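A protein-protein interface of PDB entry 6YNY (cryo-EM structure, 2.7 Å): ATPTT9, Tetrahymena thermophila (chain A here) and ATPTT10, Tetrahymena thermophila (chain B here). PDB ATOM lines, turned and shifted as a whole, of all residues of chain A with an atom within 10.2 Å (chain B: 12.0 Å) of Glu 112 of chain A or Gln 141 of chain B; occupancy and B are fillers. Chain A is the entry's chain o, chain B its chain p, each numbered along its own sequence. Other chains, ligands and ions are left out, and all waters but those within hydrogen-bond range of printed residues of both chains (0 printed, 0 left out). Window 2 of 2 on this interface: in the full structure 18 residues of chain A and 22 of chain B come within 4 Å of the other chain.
Glu 112 of chain A touches just one residue of chain B: Gln 141.
Of chain A, only Glu 112 comes within 4 Å of Gln 141 of chain B.
No residue of chain B comes within 4 Å of Gln 109 of chain A.
Of chain B, only Asn 135 (3.5 Å) comes within 4 Å of Leu 111 of chain A.
No residue of chain B comes within 4 Å of Asn 114 of chain A.
Leu 115 of chain A touches just these residues of chain B: Val 139 (3.8 Å) and Thr 140 (3.5 Å).
No residue of chain B comes within 4 Å of Cys 116 of chain A.
Of the printed residues of chain A, Asn 135 of chain B touches Gln 108, Leu 111 and Arg 118.
Printed residues of chain B within 4 Å of Gln 108 of chain A: Asn 135 (3.4 Å), Gly 142 (3.4 Å) and Arg 143 (3.3 Å).
Printed residues of chain B within 4 Å of Arg 118 of chain A: Asn 135, His 136 and His 137.
The nearest residue of chain B that does not touch Glu 112 of chain A is Thr 140 of chain B (4.2 Å).
The nearest residue of chain A that does not touch Gln 141 of chain B is Leu 111 of chain A (4.3 Å).
The nearest printed residue of chain A that does not touch His 136 of chain B is Leu 115 of chain A (5.0 Å).
The side-chain amide nitrogen of Gln 108 of chain A sits close to the side-chain amide nitrogen of Asn 135 of chain B, 3.4 Å away.
The backbone NH (N) of Arg 143 of chain B lies within hydrogen-bond range of the side-chain amide oxygen (OE1) of Gln 108 of chain A (3.3 Å).
The backbone carbonyl oxygen (O) of Gln 141 of chain B sits close to the side-chain carboxylate (OE2) of Glu 112 of chain A, at 2.6 Å.
NH1 of Arg 118 of chain A lies within hydrogen-bond range of O of Asn 135 of chain B.
NH2 of Arg 118 of chain A is in hydrogen-bond range of O of His 136 of chain B (3.1 Å).
Of the 14 printed residues of chain B, 8 touch a printed residue of chain A.
Of the 20 printed residues of chain A, 5 touch a printed residue of chain B.
Printed residues of chain A that touch a printed residue of chain B: Gln 108, Leu 111, Glu 112, Leu 115 and Arg 118.
Among the printed residues, 10 pairs touch across the chains.
Among the printed residues, no Asp or Glu carboxylate lies within 4 Å of a Lys or Arg side-chain nitrogen of the other chain.
The backbone carbonyl oxygen of Glu 112 of chain A is in hydrogen-bond range of the side-chain sulfur of Cys 116 of chain A, at 3.4 Å.
O of Leu 115 of chain A sits at hydrogen-bond distance from ND2 of Asn 119 of chain A (3.1 Å).
The backbone NH (N) of Ala 138 of chain B lies close to a ring nitrogen (ND1) of His 136 of chain B, 3.2 Å away.
Among the printed residues, pairs that only touch across the chains: Gln 108 of chain A with Gly 142 of chain B (3.4 Å), Arg 118 of chain A with His 137 of chain B (3.5 Å), Leu 111 of chain A with Asn 135 of chain B (3.5 Å), Leu 115 of chain A with Thr 140 of chain B (3.5 Å) and Leu 115 of chain A with Val 139 of chain B (3.8 Å).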
ATOM      1  N   GLY A 107     -16.208  18.652 -16.745  1.00  0.00           N
ATOM      2  CA  GLY A 107     -17.357  18.569 -17.624  1.00  0.00           C
ATOM      3  C   GLY A 107     -17.031  18.125 -19.032  1.00  0.00           C
ATOM      4  O   GLY A 107     -17.621  18.623 -19.994  1.00  0.00           O
ATOM      5  N   GLN A 108     -16.100  17.183 -19.169  1.00  0.00           N
ATOM      6  CA  GLN A 108     -15.707  16.670 -20.471  1.00  0.00           C
ATOM      7  C   GLN A 108     -15.902  15.171 -20.628  1.00  0.00           C
ATOM      8  O   GLN A 108     -15.798  14.672 -21.753  1.00  0.00           O
ATOM      9  CB  GLN A 108     -14.238  17.013 -20.757  1.00  0.00           C
ATOM     10  CG  GLN A 108     -13.983  18.496 -20.926  1.00  0.00           C
ATOM     11  CD  GLN A 108     -14.754  19.090 -22.080  1.00  0.00           C
ATOM     12  OE1 GLN A 108     -14.743  18.560 -23.190  1.00  0.00           O
ATOM     13  NE2 GLN A 108     -15.444  20.189 -21.824  1.00  0.00           N
ATOM     14  N   GLN A 109     -16.176  14.444 -19.552  1.00  0.00           N
ATOM     15  CA  GLN A 109     -16.447  13.019 -19.640  1.00  0.00           C
ATOM     16  C   GLN A 109     -17.917  12.792 -19.959  1.00  0.00           C
ATOM     17  O   GLN A 109     -18.795  13.474 -19.425  1.00  0.00           O
ATOM     18  CB  GLN A 109     -16.076  12.318 -18.335  1.00  0.00           C
ATOM     19  CG  GLN A 109     -14.633  12.533 -17.919  1.00  0.00           C
ATOM     20  CD  GLN A 109     -13.648  12.111 -18.990  1.00  0.00           C
ATOM     21  OE1 GLN A 109     -13.949  11.258 -19.826  1.00  0.00           O
ATOM     22  NE2 GLN A 109     -12.467  12.714 -18.977  1.00  0.00           N
ATOM     23  N   GLY A 110     -18.179  11.830 -20.840  1.00  0.00           N
ATOM     24  CA  GLY A 110     -19.536  11.592 -21.284  1.00  0.00           C
ATOM     25  C   GLY A 110     -20.112  12.730 -22.089  1.00  0.00           C
ATOM     26  O   GLY A 110     -21.330  12.928 -22.092  1.00  0.00           O
ATOM     27  N   LEU A 111     -19.262  13.492 -22.772  1.00  0.00           N
ATOM     28  CA  LEU A 111     -19.706  14.658 -23.521  1.00  0.00           C
ATOM     29  C   LEU A 111     -20.117  14.307 -24.942  1.00  0.00           C
ATOM     30  O   LEU A 111     -21.053  14.905 -25.482  1.00  0.00           O
ATOM     31  CB  LEU A 111     -18.592  15.704 -23.550  1.00  0.00           C
ATOM     32  CG  LEU A 111     -18.925  17.041 -24.200  1.00  0.00           C
ATOM     33  CD1 LEU A 111     -19.939  17.789 -23.365  1.00  0.00           C
ATOM     34  CD2 LEU A 111     -17.669  17.854 -24.376  1.00  0.00           C
ATOM     35  N   GLU A 112     -19.432  13.345 -25.561  1.00  0.00           N
ATOM     36  CA  GLU A 112     -19.737  12.997 -26.943  1.00  0.00           C
ATOM     37  C   GLU A 112     -21.180  12.539 -27.097  1.00  0.00           C
ATOM     38  O   GLU A 112     -21.797  12.772 -28.141  1.00  0.00           O
ATOM     39  CB  GLU A 112     -18.785  11.908 -27.437  1.00  0.00           C
ATOM     40  CG  GLU A 112     -17.320  12.317 -27.471  1.00  0.00           C
ATOM     41  CD  GLU A 112     -16.640  12.209 -26.119  1.00  0.00           C
ATOM     42  OE1 GLU A 112     -17.329  11.891 -25.127  1.00  0.00           O
ATOM     43  OE2 GLU A 112     -15.414  12.436 -26.049  1.00  0.00           O
ATOM     44  N   GLN A 113     -21.734  11.891 -26.072  1.00  0.00           N
ATOM     45  CA  GLN A 113     -23.108  11.412 -26.161  1.00  0.00           C
ATOM     46  C   GLN A 113     -24.102  12.562 -26.087  1.00  0.00           C
ATOM     47  O   GLN A 113     -25.092  12.582 -26.826  1.00  0.00           O
ATOM     48  CB  GLN A 113     -23.378  10.399 -25.052  1.00  0.00           C
ATOM     49  CG  GLN A 113     -24.787   9.833 -25.046  1.00  0.00           C
ATOM     50  CD  GLN A 113     -25.137   9.114 -26.333  1.00  0.00           C
ATOM     51  OE1 GLN A 113     -24.263   8.805 -27.143  1.00  0.00           O
ATOM     52  NE2 GLN A 113     -26.419   8.843 -26.526  1.00  0.00           N
ATOM     53  N   ASN A 114     -23.858  13.530 -25.203  1.00  0.00           N
ATOM     54  CA  ASN A 114     -24.790  14.639 -25.051  1.00  0.00           C
ATOM     55  C   ASN A 114     -24.818  15.522 -26.290  1.00  0.00           C
ATOM     56  O   ASN A 114     -25.873  16.059 -26.644  1.00  0.00           O
ATOM     57  CB  ASN A 114     -24.424  15.466 -23.823  1.00  0.00           C
ATOM     58  CG  ASN A 114     -24.388  14.641 -22.560  1.00  0.00           C
ATOM     59  OD1 ASN A 114     -24.214  13.424 -22.604  1.00  0.00           O
ATOM     60  ND2 ASN A 114     -24.556  15.298 -21.423  1.00  0.00           N
ATOM     61  N   LEU A 115     -23.675  15.687 -26.956  1.00  0.00           N
ATOM     62  CA  LEU A 115     -23.643  16.501 -28.165  1.00  0.00           C
ATOM     63  C   LEU A 115     -24.441  15.851 -29.285  1.00  0.00           C
ATOM     64  O   LEU A 115     -25.104  16.543 -30.066  1.00  0.00           O
ATOM     65  CB  LEU A 115     -22.199  16.730 -28.601  1.00  0.00           C
ATOM     66  CG  LEU A 115     -21.303  17.433 -27.583  1.00  0.00           C
ATOM     67  CD1 LEU A 115     -19.889  17.538 -28.109  1.00  0.00           C
ATOM     68  CD2 LEU A 115     -21.843  18.804 -27.236  1.00  0.00           C
ATOM     69  N   CYS A 116     -24.389  14.522 -29.383  1.00  0.00           N
ATOM     70  CA  CYS A 116     -25.191  13.831 -30.384  1.00  0.00           C
ATOM     71  C   CYS A 116     -26.677  14.015 -30.114  1.00  0.00           C
ATOM     72  O   CYS A 116     -27.468  14.196 -31.047  1.00  0.00           O
ATOM     73  CB  CYS A 116     -24.830  12.348 -30.407  1.00  0.00           C
ATOM     74  SG  CYS A 116     -23.213  11.991 -31.123  1.00  0.00           S
ATOM     75  N   LEU A 117     -27.076  13.980 -28.842  1.00  0.00           N
ATOM     76  CA  LEU A 117     -28.471  14.223 -28.503  1.00  0.00           C
ATOM     77  C   LEU A 117     -28.872  15.649 -28.841  1.00  0.00           C
ATOM     78  O   LEU A 117     -29.976  15.889 -29.344  1.00  0.00           O
ATOM     79  CB  LEU A 117     -28.705  13.950 -27.021  1.00  0.00           C
ATOM     80  CG  LEU A 117     -28.392  12.546 -26.510  1.00  0.00           C
ATOM     81  CD1 LEU A 117     -28.504  12.518 -25.008  1.00  0.00           C
ATOM     82  CD2 LEU A 117     -29.317  11.525 -27.124  1.00  0.00           C
ATOM     83  N   ARG A 118     -27.988  16.609 -28.573  1.00  0.00           N
ATOM     84  CA  ARG A 118     -28.306  18.002 -28.857  1.00  0.00           C
ATOM     85  C   ARG A 118     -28.420  18.243 -30.354  1.00  0.00           C
ATOM     86  O   ARG A 118     -29.306  18.979 -30.804  1.00  0.00           O
ATOM     87  CB  ARG A 118     -27.243  18.908 -28.244  1.00  0.00           C
ATOM     88  CG  ARG A 118     -27.596  20.370 -28.278  1.00  0.00           C
ATOM     89  CD  ARG A 118     -26.534  21.204 -27.607  1.00  0.00           C
ATOM     90  NE  ARG A 118     -25.263  21.130 -28.312  1.00  0.00           N
ATOM     91  CZ  ARG A 118     -24.174  21.803 -27.959  1.00  0.00           C
ATOM     92  NH1 ARG A 118     -24.196  22.603 -26.906  1.00  0.00           N
ATOM     93  NH2 ARG A 118     -23.062  21.671 -28.662  1.00  0.00           N
ATOM     94  N   ASN A 119     -27.536  17.632 -31.142  1.00  0.00           N
ATOM     95  CA  ASN A 119     -27.591  17.811 -32.585  1.00  0.00           C
ATOM     96  C   ASN A 119     -28.804  17.120 -33.188  1.00  0.00           C
ATOM     97  O   ASN A 119     -29.322  17.566 -34.217  1.00  0.00           O
ATOM     98  CB  ASN A 119     -26.308  17.289 -33.227  1.00  0.00           C
ATOM     99  CG  ASN A 119     -25.084  18.067 -32.791  1.00  0.00           C
ATOM    100  OD1 ASN A 119     -25.166  19.256 -32.487  1.00  0.00           O
ATOM    101  ND2 ASN A 119     -23.938  17.398 -32.757  1.00  0.00           N
ATOM    102  N   CYS A 120     -29.273  16.037 -32.566  1.00  0.00           N
ATOM    103  CA  CYS A 120     -30.469  15.368 -33.062  1.00  0.00           C
ATOM    104  C   CYS A 120     -31.714  16.206 -32.810  1.00  0.00           C
ATOM    105  O   CYS A 120     -32.615  16.257 -33.653  1.00  0.00           O
ATOM    106  CB  CYS A 120     -30.616  13.996 -32.406  1.00  0.00           C
ATOM    107  SG  CYS A 120     -29.469  12.718 -32.979  1.00  0.00           S
ATOM    108  N   LEU A 133     -31.775   9.703 -33.168  1.00  0.00           N
ATOM    109  CA  LEU A 133     -31.399   9.078 -31.906  1.00  0.00           C
ATOM    110  C   LEU A 133     -31.181   7.581 -32.075  1.00  0.00           C
ATOM    111  O   LEU A 133     -30.238   7.018 -31.509  1.00  0.00           O
ATOM    112  CB  LEU A 133     -32.475   9.340 -30.857  1.00  0.00           C
ATOM    113  CG  LEU A 133     -32.735  10.807 -30.523  1.00  0.00           C
ATOM    114  CD1 LEU A 133     -33.922  10.928 -29.600  1.00  0.00           C
ATOM    115  CD2 LEU A 133     -31.513  11.444 -29.899  1.00  0.00           C
ATOM    116  N   LYS A 136     -27.878   7.390 -34.608  1.00  0.00           N
ATOM    117  CA  LYS A 136     -26.611   7.986 -34.205  1.00  0.00           C
ATOM    118  C   LYS A 136     -26.322   7.876 -32.718  1.00  0.00           C
ATOM    119  O   LYS A 136     -25.153   7.782 -32.339  1.00  0.00           O
ATOM    120  CB  LYS A 136     -26.573   9.468 -34.594  1.00  0.00           C
ATOM    121  CG  LYS A 136     -26.735   9.743 -36.080  1.00  0.00           C
ATOM    122  CD  LYS A 136     -25.628   9.133 -36.925  1.00  0.00           C
ATOM    123  CE  LYS A 136     -24.257   9.693 -36.581  1.00  0.00           C
ATOM    124  NZ  LYS A 136     -24.199  11.174 -36.670  1.00  0.00           N
ATOM    125  N   CYS A 137     -27.347   7.889 -31.867  1.00  0.00           N
ATOM    126  CA  CYS A 137     -27.168   7.912 -30.423  1.00  0.00           C
ATOM    127  C   CYS A 137     -27.313   6.534 -29.789  1.00  0.00           C
ATOM    128  O   CYS A 137     -27.488   6.435 -28.570  1.00  0.00           O
ATOM    129  CB  CYS A 137     -28.158   8.886 -29.789  1.00  0.00           C
ATOM    130  SG  CYS A 137     -27.963  10.593 -30.336  1.00  0.00           S
ATOM    131  N   GLY A 138     -27.243   5.474 -30.584  1.00  0.00           N
ATOM    132  CA  GLY A 138     -27.284   4.127 -30.044  1.00  0.00           C
ATOM    133  C   GLY A 138     -28.616   3.720 -29.453  1.00  0.00           C
ATOM    134  O   GLY A 138     -28.648   3.042 -28.418  1.00  0.00           O
ATOM    135  N   ILE A 148     -32.440  14.676 -20.109  1.00  0.00           N
ATOM    136  CA  ILE A 148     -31.008  14.883 -19.943  1.00  0.00           C
ATOM    137  C   ILE A 148     -30.618  16.279 -20.404  1.00  0.00           C
ATOM    138  O   ILE A 148     -29.825  16.967 -19.751  1.00  0.00           O
ATOM    139  CB  ILE A 148     -30.231  13.799 -20.706  1.00  0.00           C
ATOM    140  CG1 ILE A 148     -30.571  12.417 -20.149  1.00  0.00           C
ATOM    141  CG2 ILE A 148     -28.740  14.062 -20.630  1.00  0.00           C
ATOM    142  CD1 ILE A 148     -30.041  11.284 -20.978  1.00  0.00           C
ATOM    143  N   LEU A 149     -31.166  16.717 -21.534  1.00  0.00           N
ATOM    144  CA  LEU A 149     -30.860  18.035 -22.068  1.00  0.00           C
ATOM    145  C   LEU A 149     -31.578  19.152 -21.329  1.00  0.00           C
ATOM    146  O   LEU A 149     -31.151  20.309 -21.417  1.00  0.00           O
ATOM    147  CB  LEU A 149     -31.229  18.083 -23.548  1.00  0.00           C
ATOM    148  CG  LEU A 149     -30.589  17.003 -24.413  1.00  0.00           C
ATOM    149  CD1 LEU A 149     -31.147  17.058 -25.810  1.00  0.00           C
ATOM    150  CD2 LEU A 149     -29.092  17.166 -24.437  1.00  0.00           C
ATOM    151  N   TYR B 108      -0.330  18.433 -19.223  1.00  0.00           N
ATOM    152  CA  TYR B 108      -0.230  17.841 -20.543  1.00  0.00           C
ATOM    153  C   TYR B 108       1.201  17.385 -20.771  1.00  0.00           C
ATOM    154  O   TYR B 108       2.142  17.898 -20.163  1.00  0.00           O
ATOM    155  CB  TYR B 108      -0.658  18.829 -21.632  1.00  0.00           C
ATOM    156  CG  TYR B 108      -2.062  19.352 -21.466  1.00  0.00           C
ATOM    157  CD1 TYR B 108      -3.115  18.804 -22.176  1.00  0.00           C
ATOM    158  CD2 TYR B 108      -2.337  20.390 -20.591  1.00  0.00           C
ATOM    159  CE1 TYR B 108      -4.396  19.277 -22.025  1.00  0.00           C
ATOM    160  CE2 TYR B 108      -3.614  20.867 -20.434  1.00  0.00           C
ATOM    161  CZ  TYR B 108      -4.641  20.308 -21.152  1.00  0.00           C
ATOM    162  OH  TYR B 108      -5.917  20.787 -20.994  1.00  0.00           O
ATOM    163  N   GLU B 113       0.042  21.169 -26.487  1.00  0.00           N
ATOM    164  CA  GLU B 113      -1.305  20.750 -26.133  1.00  0.00           C
ATOM    165  C   GLU B 113      -1.917  21.594 -25.026  1.00  0.00           C
ATOM    166  O   GLU B 113      -3.096  21.410 -24.710  1.00  0.00           O
ATOM    167  CB  GLU B 113      -1.297  19.286 -25.693  1.00  0.00           C
ATOM    168  CG  GLU B 113      -0.763  18.324 -26.731  1.00  0.00           C
ATOM    169  CD  GLU B 113      -0.705  16.897 -26.226  1.00  0.00           C
ATOM    170  OE1 GLU B 113      -0.899  16.685 -25.012  1.00  0.00           O
ATOM    171  OE2 GLU B 113      -0.467  15.985 -27.046  1.00  0.00           O
ATOM    172  N   LEU B 134     -18.060  26.014 -22.944  1.00  0.00           N
ATOM    173  CA  LEU B 134     -17.111  25.582 -23.957  1.00  0.00           C
ATOM    174  C   LEU B 134     -17.730  24.621 -24.959  1.00  0.00           C
ATOM    175  O   LEU B 134     -17.203  24.477 -26.066  1.00  0.00           O
ATOM    176  CB  LEU B 134     -15.913  24.906 -23.298  1.00  0.00           C
ATOM    177  CG  LEU B 134     -15.041  25.762 -22.386  1.00  0.00           C
ATOM    178  CD1 LEU B 134     -14.053  24.892 -21.657  1.00  0.00           C
ATOM    179  CD2 LEU B 134     -14.316  26.820 -23.175  1.00  0.00           C
ATOM    180  N   ASN B 135     -18.830  23.965 -24.595  1.00  0.00           N
ATOM    181  CA  ASN B 135     -19.460  22.957 -25.442  1.00  0.00           C
ATOM    182  C   ASN B 135     -20.360  23.643 -26.467  1.00  0.00           C
ATOM    183  O   ASN B 135     -21.585  23.504 -26.472  1.00  0.00           O
ATOM    184  CB  ASN B 135     -20.240  21.967 -24.590  1.00  0.00           C
ATOM    185  CG  ASN B 135     -19.490  21.554 -23.342  1.00  0.00           C
ATOM    186  OD1 ASN B 135     -20.034  21.585 -22.240  1.00  0.00           O
ATOM    187  ND2 ASN B 135     -18.235  21.170 -23.506  1.00  0.00           N
ATOM    188  N   HIS B 136     -19.724  24.403 -27.351  1.00  0.00           N
ATOM    189  CA  HIS B 136     -20.471  25.108 -28.377  1.00  0.00           C
ATOM    190  C   HIS B 136     -20.893  24.147 -29.483  1.00  0.00           C
ATOM    191  O   HIS B 136     -20.419  23.013 -29.583  1.00  0.00           O
ATOM    192  CB  HIS B 136     -19.660  26.273 -28.939  1.00  0.00           C
ATOM    193  CG  HIS B 136     -18.299  25.895 -29.423  1.00  0.00           C
ATOM    194  ND1 HIS B 136     -18.076  25.356 -30.671  1.00  0.00           N
ATOM    195  CD2 HIS B 136     -17.087  25.988 -28.832  1.00  0.00           C
ATOM    196  CE1 HIS B 136     -16.785  25.129 -30.824  1.00  0.00           C
ATOM    197  NE2 HIS B 136     -16.163  25.503 -29.723  1.00  0.00           N
ATOM    198  N   HIS B 137     -21.807  24.620 -30.325  1.00  0.00           N
ATOM    199  CA  HIS B 137     -22.450  23.788 -31.331  1.00  0.00           C
ATOM    200  C   HIS B 137     -21.510  23.337 -32.435  1.00  0.00           C
ATOM    201  O   HIS B 137     -21.944  22.594 -33.320  1.00  0.00           O
ATOM    202  CB  HIS B 137     -23.634  24.542 -31.927  1.00  0.00           C
ATOM    203  CG  HIS B 137     -24.750  24.759 -30.958  1.00  0.00           C
ATOM    204  ND1 HIS B 137     -24.617  25.545 -29.835  1.00  0.00           N
ATOM    205  CD2 HIS B 137     -26.015  24.279 -30.933  1.00  0.00           C
ATOM    206  CE1 HIS B 137     -25.756  25.547 -29.165  1.00  0.00           C
ATOM    207  NE2 HIS B 137     -26.620  24.786 -29.811  1.00  0.00           N
ATOM    208  N   ALA B 138     -20.250  23.760 -32.411  1.00  0.00           N
ATOM    209  CA  ALA B 138     -19.241  23.276 -33.338  1.00  0.00           C
ATOM    210  C   ALA B 138     -18.275  22.299 -32.685  1.00  0.00           C
ATOM    211  O   ALA B 138     -17.296  21.893 -33.317  1.00  0.00           O
ATOM    212  CB  ALA B 138     -18.477  24.452 -33.938  1.00  0.00           C
ATOM    213  N   VAL B 139     -18.529  21.916 -31.441  1.00  0.00           N
ATOM    214  CA  VAL B 139     -17.694  20.952 -30.739  1.00  0.00           C
ATOM    215  C   VAL B 139     -18.071  19.544 -31.171  1.00  0.00           C
ATOM    216  O   VAL B 139     -19.229  19.256 -31.491  1.00  0.00           O
ATOM    217  CB  VAL B 139     -17.841  21.131 -29.215  1.00  0.00           C
ATOM    218  CG1 VAL B 139     -17.070  20.070 -28.478  1.00  0.00           C
ATOM    219  CG2 VAL B 139     -17.368  22.497 -28.807  1.00  0.00           C
ATOM    220  N   THR B 140     -17.078  18.655 -31.184  1.00  0.00           N
ATOM    221  CA  THR B 140     -17.277  17.278 -31.618  1.00  0.00           C
ATOM    222  C   THR B 140     -16.989  16.268 -30.515  1.00  0.00           C
ATOM    223  O   THR B 140     -17.887  15.509 -30.140  1.00  0.00           O
ATOM    224  CB  THR B 140     -16.401  16.987 -32.843  1.00  0.00           C
ATOM    225  OG1 THR B 140     -15.028  17.239 -32.527  1.00  0.00           O
ATOM    226  CG2 THR B 140     -16.815  17.853 -34.014  1.00  0.00           C
ATOM    227  N   GLN B 141     -15.768  16.230 -29.982  1.00  0.00           N
ATOM    228  CA  GLN B 141     -15.330  15.130 -29.132  1.00  0.00           C
ATOM    229  C   GLN B 141     -15.099  15.516 -27.679  1.00  0.00           C
ATOM    230  O   GLN B 141     -15.671  14.892 -26.782  1.00  0.00           O
ATOM    231  CB  GLN B 141     -14.051  14.515 -29.719  1.00  0.00           C
ATOM    232  CG  GLN B 141     -12.961  15.514 -30.057  1.00  0.00           C
ATOM    233  CD  GLN B 141     -11.710  14.847 -30.581  1.00  0.00           C
ATOM    234  OE1 GLN B 141     -11.677  13.636 -30.790  1.00  0.00           O
ATOM    235  NE2 GLN B 141     -10.668  15.637 -30.794  1.00  0.00           N
ATOM    236  N   GLY B 142     -14.290  16.525 -27.410  1.00  0.00           N
ATOM    237  CA  GLY B 142     -13.942  16.867 -26.047  1.00  0.00           C
ATOM    238  C   GLY B 142     -12.525  17.401 -25.969  1.00  0.00           C
ATOM    239  O   GLY B 142     -11.883  17.663 -26.980  1.00  0.00           O
ATOM    240  N   ARG B 143     -12.053  17.551 -24.730  1.00  0.00           N
ATOM    241  CA  ARG B 143     -10.727  18.096 -24.446  1.00  0.00           C
ATOM    242  C   ARG B 143      -9.695  17.009 -24.162  1.00  0.00           C
ATOM    243  O   ARG B 143      -8.661  16.940 -24.831  1.00  0.00           O
ATOM    244  CB  ARG B 143     -10.828  19.065 -23.265  1.00  0.00           C
ATOM    245  CG  ARG B 143     -11.865  20.161 -23.469  1.00  0.00           C
ATOM    246  CD  ARG B 143     -11.442  21.160 -24.525  1.00  0.00           C
ATOM    247  NE  ARG B 143     -12.545  22.032 -24.916  1.00  0.00           N
ATOM    248  CZ  ARG B 143     -12.442  23.025 -25.790  1.00  0.00           C
ATOM    249  NH1 ARG B 143     -11.280  23.289 -26.372  1.00  0.00           N
ATOM    250  NH2 ARG B 143     -13.506  23.758 -26.082  1.00  0.00           N
ATOM    251  N   GLN B 144      -9.960  16.156 -23.173  1.00  0.00           N
ATOM    252  CA  GLN B 144      -9.135  14.982 -22.884  1.00  0.00           C
ATOM    253  C   GLN B 144      -7.688  15.378 -22.570  1.00  0.00           C
ATOM    254  O   GLN B 144      -6.753  15.106 -23.323  1.00  0.00           O
ATOM    255  CB  GLN B 144      -9.191  13.989 -24.053  1.00  0.00           C
ATOM    256  CG  GLN B 144      -8.692  12.590 -23.718  1.00  0.00           C
ATOM    257  CD  GLN B 144      -7.199  12.422 -23.930  1.00  0.00           C
ATOM    258  OE1 GLN B 144      -6.610  13.049 -24.811  1.00  0.00           O
ATOM    259  NE2 GLN B 144      -6.578  11.576 -23.118  1.00  0.00           N
ATOM    260  N   TYR B 145      -7.533  16.061 -21.439  1.00  0.00           N
ATOM    261  CA  TYR B 145      -6.204  16.340 -20.917  1.00  0.00           C
ATOM    262  C   TYR B 145      -5.553  15.046 -20.429  1.00  0.00           C
ATOM    263  O   TYR B 145      -6.128  13.958 -20.503  1.00  0.00           O
ATOM    264  CB  TYR B 145      -6.268  17.376 -19.797  1.00  0.00           C
ATOM    265  CG  TYR B 145      -7.074  16.961 -18.590  1.00  0.00           C
ATOM    266  CD1 TYR B 145      -8.383  17.383 -18.429  1.00  0.00           C
ATOM    267  CD2 TYR B 145      -6.522  16.159 -17.606  1.00  0.00           C
ATOM    268  CE1 TYR B 145      -9.120  17.011 -17.328  1.00  0.00           C
ATOM    269  CE2 TYR B 145      -7.252  15.780 -16.503  1.00  0.00           C
ATOM    270  CZ  TYR B 145      -8.551  16.210 -16.369  1.00  0.00           C
ATOM    271  OH  TYR B 145      -9.289  15.839 -15.269  1.00  0.00           O
